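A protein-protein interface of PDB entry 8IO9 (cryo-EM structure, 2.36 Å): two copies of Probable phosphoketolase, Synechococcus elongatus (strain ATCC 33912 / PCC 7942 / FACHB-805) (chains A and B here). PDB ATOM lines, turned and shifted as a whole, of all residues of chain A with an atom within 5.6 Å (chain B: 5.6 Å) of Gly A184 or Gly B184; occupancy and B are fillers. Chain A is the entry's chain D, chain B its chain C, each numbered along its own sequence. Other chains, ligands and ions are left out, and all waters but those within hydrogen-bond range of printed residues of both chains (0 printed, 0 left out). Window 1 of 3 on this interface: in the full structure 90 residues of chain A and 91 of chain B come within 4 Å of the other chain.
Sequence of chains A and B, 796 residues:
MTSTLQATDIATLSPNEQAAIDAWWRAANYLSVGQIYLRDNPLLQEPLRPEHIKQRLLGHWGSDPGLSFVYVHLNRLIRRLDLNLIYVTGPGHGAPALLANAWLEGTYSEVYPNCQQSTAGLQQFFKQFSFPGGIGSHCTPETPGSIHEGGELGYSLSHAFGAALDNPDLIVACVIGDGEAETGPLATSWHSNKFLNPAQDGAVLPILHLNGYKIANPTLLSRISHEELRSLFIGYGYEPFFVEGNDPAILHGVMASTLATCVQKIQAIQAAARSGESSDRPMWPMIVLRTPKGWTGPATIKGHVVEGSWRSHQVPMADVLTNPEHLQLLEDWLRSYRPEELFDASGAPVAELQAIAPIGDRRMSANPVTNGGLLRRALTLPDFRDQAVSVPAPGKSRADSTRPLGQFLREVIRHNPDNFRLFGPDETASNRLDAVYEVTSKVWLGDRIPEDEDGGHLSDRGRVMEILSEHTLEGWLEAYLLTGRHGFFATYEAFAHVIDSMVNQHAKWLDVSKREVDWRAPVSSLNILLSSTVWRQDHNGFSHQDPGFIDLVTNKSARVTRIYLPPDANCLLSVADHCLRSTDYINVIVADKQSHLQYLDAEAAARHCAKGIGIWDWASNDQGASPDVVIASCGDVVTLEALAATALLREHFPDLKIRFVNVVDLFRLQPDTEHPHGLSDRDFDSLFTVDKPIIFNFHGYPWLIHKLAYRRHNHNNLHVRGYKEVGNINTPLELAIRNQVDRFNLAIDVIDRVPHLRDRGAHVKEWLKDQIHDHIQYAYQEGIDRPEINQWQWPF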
ATOM      1  N   GLU A 182       9.367  10.112 -22.969  1.00  0.00           N
ATOM      2  CA  GLU A 182      10.409   9.161 -23.337  1.00  0.00           C
ATOM      3  C   GLU A 182      11.590   9.820 -24.038  1.00  0.00           C
ATOM      4  O   GLU A 182      12.646   9.191 -24.156  1.00  0.00           O
ATOM      5  CB  GLU A 182       9.831   8.064 -24.231  1.00  0.00           C
ATOM      6  CG  GLU A 182       8.660   7.314 -23.622  1.00  0.00           C
ATOM      7  CD  GLU A 182       8.178   6.177 -24.502  1.00  0.00           C
ATOM      8  OE1 GLU A 182       8.694   6.035 -25.630  1.00  0.00           O
ATOM      9  OE2 GLU A 182       7.283   5.424 -24.067  1.00  0.00           O
ATOM     10  N   THR A 183      11.443  11.056 -24.502  1.00  0.00           N
ATOM     11  CA  THR A 183      12.524  11.736 -25.193  1.00  0.00           C
ATOM     12  C   THR A 183      13.593  12.188 -24.208  1.00  0.00           C
ATOM     13  O   THR A 183      13.320  12.441 -23.032  1.00  0.00           O
ATOM     14  CB  THR A 183      11.998  12.943 -25.967  1.00  0.00           C
ATOM     15  OG1 THR A 183      11.281  13.807 -25.078  1.00  0.00           O
ATOM     16  CG2 THR A 183      11.072  12.495 -27.080  1.00  0.00           C
ATOM     17  N   GLY A 184      14.820  12.293 -24.706  1.00  0.00           N
ATOM     18  CA  GLY A 184      15.955  12.677 -23.902  1.00  0.00           C
ATOM     19  C   GLY A 184      15.864  14.057 -23.282  1.00  0.00           C
ATOM     20  O   GLY A 184      16.057  14.222 -22.075  1.00  0.00           O
ATOM     21  N   PRO A 185      15.582  15.080 -24.095  1.00  0.00           N
ATOM     22  CA  PRO A 185      15.489  16.442 -23.545  1.00  0.00           C
ATOM     23  C   PRO A 185      14.509  16.602 -22.396  1.00  0.00           C
ATOM     24  O   PRO A 185      14.778  17.388 -21.481  1.00  0.00           O
ATOM     25  CB  PRO A 185      15.062  17.264 -24.763  1.00  0.00           C
ATOM     26  CG  PRO A 185      15.693  16.570 -25.896  1.00  0.00           C
ATOM     27  CD  PRO A 185      15.674  15.105 -25.567  1.00  0.00           C
ATOM     28  N   LEU A 186      13.374  15.905 -22.413  1.00  0.00           N
ATOM     29  CA  LEU A 186      12.404  16.106 -21.346  1.00  0.00           C
ATOM     30  C   LEU A 186      12.724  15.282 -20.105  1.00  0.00           C
ATOM     31  O   LEU A 186      12.355  15.681 -18.995  1.00  0.00           O
ATOM     32  CB  LEU A 186      10.993  15.790 -21.839  1.00  0.00           C
ATOM     33  CG  LEU A 186       9.889  16.157 -20.846  1.00  0.00           C
ATOM     34  CD1 LEU A 186       8.649  16.588 -21.581  1.00  0.00           C
ATOM     35  CD2 LEU A 186       9.584  14.996 -19.929  1.00  0.00           C
ATOM     36  N   ALA A 187      13.396  14.141 -20.262  1.00  0.00           N
ATOM     37  CA  ALA A 187      13.730  13.325 -19.099  1.00  0.00           C
ATOM     38  C   ALA A 187      14.686  14.058 -18.167  1.00  0.00           C
ATOM     39  O   ALA A 187      14.586  13.933 -16.941  1.00  0.00           O
ATOM     40  CB  ALA A 187      14.326  11.991 -19.545  1.00  0.00           C
ATOM     41  N   THR A 188      15.612  14.831 -18.725  1.00  0.00           N
ATOM     42  CA  THR A 188      16.571  15.576 -17.921  1.00  0.00           C
ATOM     43  C   THR A 188      16.041  16.926 -17.457  1.00  0.00           C
ATOM     44  O   THR A 188      16.547  17.465 -16.468  1.00  0.00           O
ATOM     45  CB  THR A 188      17.874  15.784 -18.707  1.00  0.00           C
ATOM     46  OG1 THR A 188      18.879  16.325 -17.842  1.00  0.00           O
ATOM     47  CG2 THR A 188      17.655  16.739 -19.864  1.00  0.00           C
ATOM     48  N   SER A 189      15.037  17.484 -18.137  1.00  0.00           N
ATOM     49  CA  SER A 189      14.528  18.792 -17.752  1.00  0.00           C
ATOM     50  C   SER A 189      13.634  18.730 -16.529  1.00  0.00           C
ATOM     51  O   SER A 189      13.232  19.784 -16.028  1.00  0.00           O
ATOM     52  CB  SER A 189      13.775  19.438 -18.915  1.00  0.00           C
ATOM     53  OG  SER A 189      12.675  18.647 -19.315  1.00  0.00           O
ATOM     54  N   SER A 469      23.104  19.807 -19.041  1.00  0.00           N
ATOM     55  CA  SER A 469      22.210  19.532 -20.159  1.00  0.00           C
ATOM     56  C   SER A 469      22.044  20.790 -20.998  1.00  0.00           C
ATOM     57  O   SER A 469      21.514  21.798 -20.520  1.00  0.00           O
ATOM     58  CB  SER A 469      20.858  19.045 -19.652  1.00  0.00           C
ATOM     59  OG  SER A 469      19.932  18.949 -20.719  1.00  0.00           O
ATOM     60  N   HIS A 471      20.144  20.942 -23.682  1.00  0.00           N
ATOM     61  CA  HIS A 471      18.733  21.040 -24.041  1.00  0.00           C
ATOM     62  C   HIS A 471      17.964  21.862 -23.019  1.00  0.00           C
ATOM     63  O   HIS A 471      17.127  22.695 -23.384  1.00  0.00           O
ATOM     64  CB  HIS A 471      18.119  19.649 -24.162  1.00  0.00           C
ATOM     65  CG  HIS A 471      18.659  18.848 -25.301  1.00  0.00           C
ATOM     66  ND1 HIS A 471      19.523  17.790 -25.122  1.00  0.00           N
ATOM     67  CD2 HIS A 471      18.458  18.948 -26.635  1.00  0.00           C
ATOM     68  CE1 HIS A 471      19.829  17.273 -26.297  1.00  0.00           C
ATOM     69  NE2 HIS A 471      19.199  17.959 -27.232  1.00  0.00           N
ATOM     70  N   GLU B 182      23.648  14.216 -16.098  1.00  0.00           N
ATOM     71  CA  GLU B 182      22.793  15.386 -16.251  1.00  0.00           C
ATOM     72  C   GLU B 182      22.383  15.633 -17.697  1.00  0.00           C
ATOM     73  O   GLU B 182      21.452  16.410 -17.935  1.00  0.00           O
ATOM     74  CB  GLU B 182      23.494  16.627 -15.698  1.00  0.00           C
ATOM     75  CG  GLU B 182      23.926  16.508 -14.250  1.00  0.00           C
ATOM     76  CD  GLU B 182      24.541  17.788 -13.721  1.00  0.00           C
ATOM     77  OE1 GLU B 182      24.735  18.729 -14.517  1.00  0.00           O
ATOM     78  OE2 GLU B 182      24.830  17.854 -12.509  1.00  0.00           O
ATOM     79  N   THR B 183      23.045  15.003 -18.660  1.00  0.00           N
ATOM     80  CA  THR B 183      22.716  15.206 -20.060  1.00  0.00           C
ATOM     81  C   THR B 183      21.427  14.481 -20.420  1.00  0.00           C
ATOM     82  O   THR B 183      21.066  13.469 -19.816  1.00  0.00           O
ATOM     83  CB  THR B 183      23.849  14.716 -20.959  1.00  0.00           C
ATOM     84  OG1 THR B 183      24.146  13.348 -20.653  1.00  0.00           O
ATOM     85  CG2 THR B 183      25.092  15.554 -20.745  1.00  0.00           C
ATOM     86  N   GLY B 184      20.738  15.012 -21.426  1.00  0.00           N
ATOM     87  CA  GLY B 184      19.478  14.471 -21.876  1.00  0.00           C
ATOM     88  C   GLY B 184      19.537  13.042 -22.379  1.00  0.00           C
ATOM     89  O   GLY B 184      18.758  12.187 -21.948  1.00  0.00           O
ATOM     90  N   PRO B 185      20.452  12.754 -23.310  1.00  0.00           N
ATOM     91  CA  PRO B 185      20.544  11.385 -23.840  1.00  0.00           C
ATOM     92  C   PRO B 185      20.732  10.303 -22.790  1.00  0.00           C
ATOM     93  O   PRO B 185      20.191   9.204 -22.955  1.00  0.00           O
ATOM     94  CB  PRO B 185      21.752  11.472 -24.774  1.00  0.00           C
ATOM     95  CG  PRO B 185      21.710  12.852 -25.279  1.00  0.00           C
ATOM     96  CD  PRO B 185      21.196  13.706 -24.155  1.00  0.00           C
ATOM     97  N   LEU B 186      21.488  10.562 -21.725  1.00  0.00           N
ATOM     98  CA  LEU B 186      21.723   9.502 -20.752  1.00  0.00           C
ATOM     99  C   LEU B 186      20.589   9.376 -19.743  1.00  0.00           C
ATOM    100  O   LEU B 186      20.364   8.284 -19.211  1.00  0.00           O
ATOM    101  CB  LEU B 186      23.051   9.726 -20.029  1.00  0.00           C
ATOM    102  CG  LEU B 186      23.472   8.563 -19.130  1.00  0.00           C
ATOM    103  CD1 LEU B 186      24.971   8.435 -19.110  1.00  0.00           C
ATOM    104  CD2 LEU B 186      22.937   8.747 -17.728  1.00  0.00           C
ATOM    105  N   ALA B 187      19.870  10.464 -19.463  1.00  0.00           N
ATOM    106  CA  ALA B 187      18.767  10.386 -18.510  1.00  0.00           C
ATOM    107  C   ALA B 187      17.659   9.475 -19.023  1.00  0.00           C
ATOM    108  O   ALA B 187      17.028   8.754 -18.243  1.00  0.00           O
ATOM    109  CB  ALA B 187      18.226  11.784 -18.217  1.00  0.00           C
ATOM    110  N   THR B 188      17.412   9.489 -20.331  1.00  0.00           N
ATOM    111  CA  THR B 188      16.375   8.655 -20.918  1.00  0.00           C
ATOM    112  C   THR B 188      16.856   7.248 -21.249  1.00  0.00           C
ATOM    113  O   THR B 188      16.028   6.339 -21.364  1.00  0.00           O
ATOM    114  CB  THR B 188      15.821   9.314 -22.189  1.00  0.00           C
ATOM    115  OG1 THR B 188      14.660   8.606 -22.637  1.00  0.00           O
ATOM    116  CG2 THR B 188      16.859   9.304 -23.295  1.00  0.00           C
ATOM    117  N   SER B 189      18.165   7.043 -21.400  1.00  0.00           N
ATOM    118  CA  SER B 189      18.663   5.725 -21.765  1.00  0.00           C
ATOM    119  C   SER B 189      18.699   4.770 -20.586  1.00  0.00           C
ATOM    120  O   SER B 189      18.999   3.590 -20.780  1.00  0.00           O
ATOM    121  CB  SER B 189      20.055   5.831 -22.390  1.00  0.00           C
ATOM    122  OG  SER B 189      20.977   6.408 -21.490  1.00  0.00           O
ATOM    123  N   SER B 469      12.729   7.803 -27.827  1.00  0.00           N
ATOM    124  CA  SER B 469      13.997   8.520 -27.750  1.00  0.00           C
ATOM    125  C   SER B 469      14.883   8.111 -28.916  1.00  0.00           C
ATOM    126  O   SER B 469      15.276   6.946 -29.028  1.00  0.00           O
ATOM    127  CB  SER B 469      14.691   8.233 -26.425  1.00  0.00           C
ATOM    128  OG  SER B 469      15.997   8.781 -26.418  1.00  0.00           O
ATOM    129  N   HIS B 471      17.931   9.298 -29.382  1.00  0.00           N
ATOM    130  CA  HIS B 471      19.285   9.132 -28.865  1.00  0.00           C
ATOM    131  C   HIS B 471      19.531   7.695 -28.435  1.00  0.00           C
ATOM    132  O   HIS B 471      20.595   7.127 -28.702  1.00  0.00           O
ATOM    133  CB  HIS B 471      19.525  10.081 -27.693  1.00  0.00           C
ATOM    134  CG  HIS B 471      19.532  11.525 -28.077  1.00  0.00           C
ATOM    135  ND1 HIS B 471      18.499  12.381 -27.767  1.00  0.00           N
ATOM    136  CD2 HIS B 471      20.449  12.266 -28.741  1.00  0.00           C
ATOM    137  CE1 HIS B 471      18.779  13.587 -28.226  1.00  0.00           C
ATOM    138  NE2 HIS B 471      19.955  13.544 -28.823  1.00  0.00           N
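Printed residues of chain B within 4 Å of Gly A184: Gly B184 (3.4 Å) and Thr B188 (3.5 Å).
Of chain A, only Gly A184 (3.4 Å) and Thr A188 (3.5 Å) come within 4 Å of Gly B184.
Of the printed residues of chain A, Thr B188 touches Glu A182 (2.6 Å) and Gly A184 (3.5 Å).
Of the printed residues of chain B, Ser A469 touches Glu B182.
Of the printed residues of chain A, Ser B469 touches Glu A182.
Pro B185 touches none of the printed residues of chain A.
The nearest residue of chain B that does not touch Gly A184 is Ser B469 (4.1 Å).
The nearest printed residue of chain B that does not touch Thr A188 is Ala B187 (4.05 Å).
The backbone carbonyl oxygen (O) of Gly A184 lies close to the backbone carbonyl oxygen (O) of Gly B184 (3.4 Å).
OG1 of Thr A188 sits at hydrogen-bond distance from O of Glu B182, 2.6 Å away.
The side-chain hydroxyl (OG1) of Thr B188 sits at hydrogen-bond distance from the backbone carbonyl oxygen (O) of Glu A182 (2.6 Å).
Glu A182 touches Thr B188, and with the chains exchanged Thr A188 touches Glu B182.
Glu A182 touches Ser B469, and with the chains exchanged Ser A469 touches Glu B182.
Gly B184 touches its own counterpart, Gly A184.
Gly A184 touches Thr B188, and with the chains exchanged Thr A188 touches Gly B184.
10 positions are printed for both chains.
Of the 7 pairs that touch across the chains among the printed residues, 7 have their exchanged pair printed and touching as well.
Among the printed residues, merely in contact across the chains: Ser A469 with Glu B182 (3.2 Å), Glu A182 with Ser B469 (3.2 Å), Thr A188 with Gly B184 (3.5 Å) and Gly A184 with Thr B188 (3.5 Å).
Of the 10 printed residues of chain A, 4 touch a printed residue of chain B.
Printed residues of chain A that touch a printed residue of chain B: Glu A182, Gly A184, Thr A188 and Ser A469.
Printed residues of chain B that touch a printed residue of chain A: Glu B182, Gly B184, Thr B188 and Ser B469.
Among the printed residues, no Asp or Glu carboxylate lies within 4 Å of a Lys or Arg side-chain nitrogen of the other chain.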
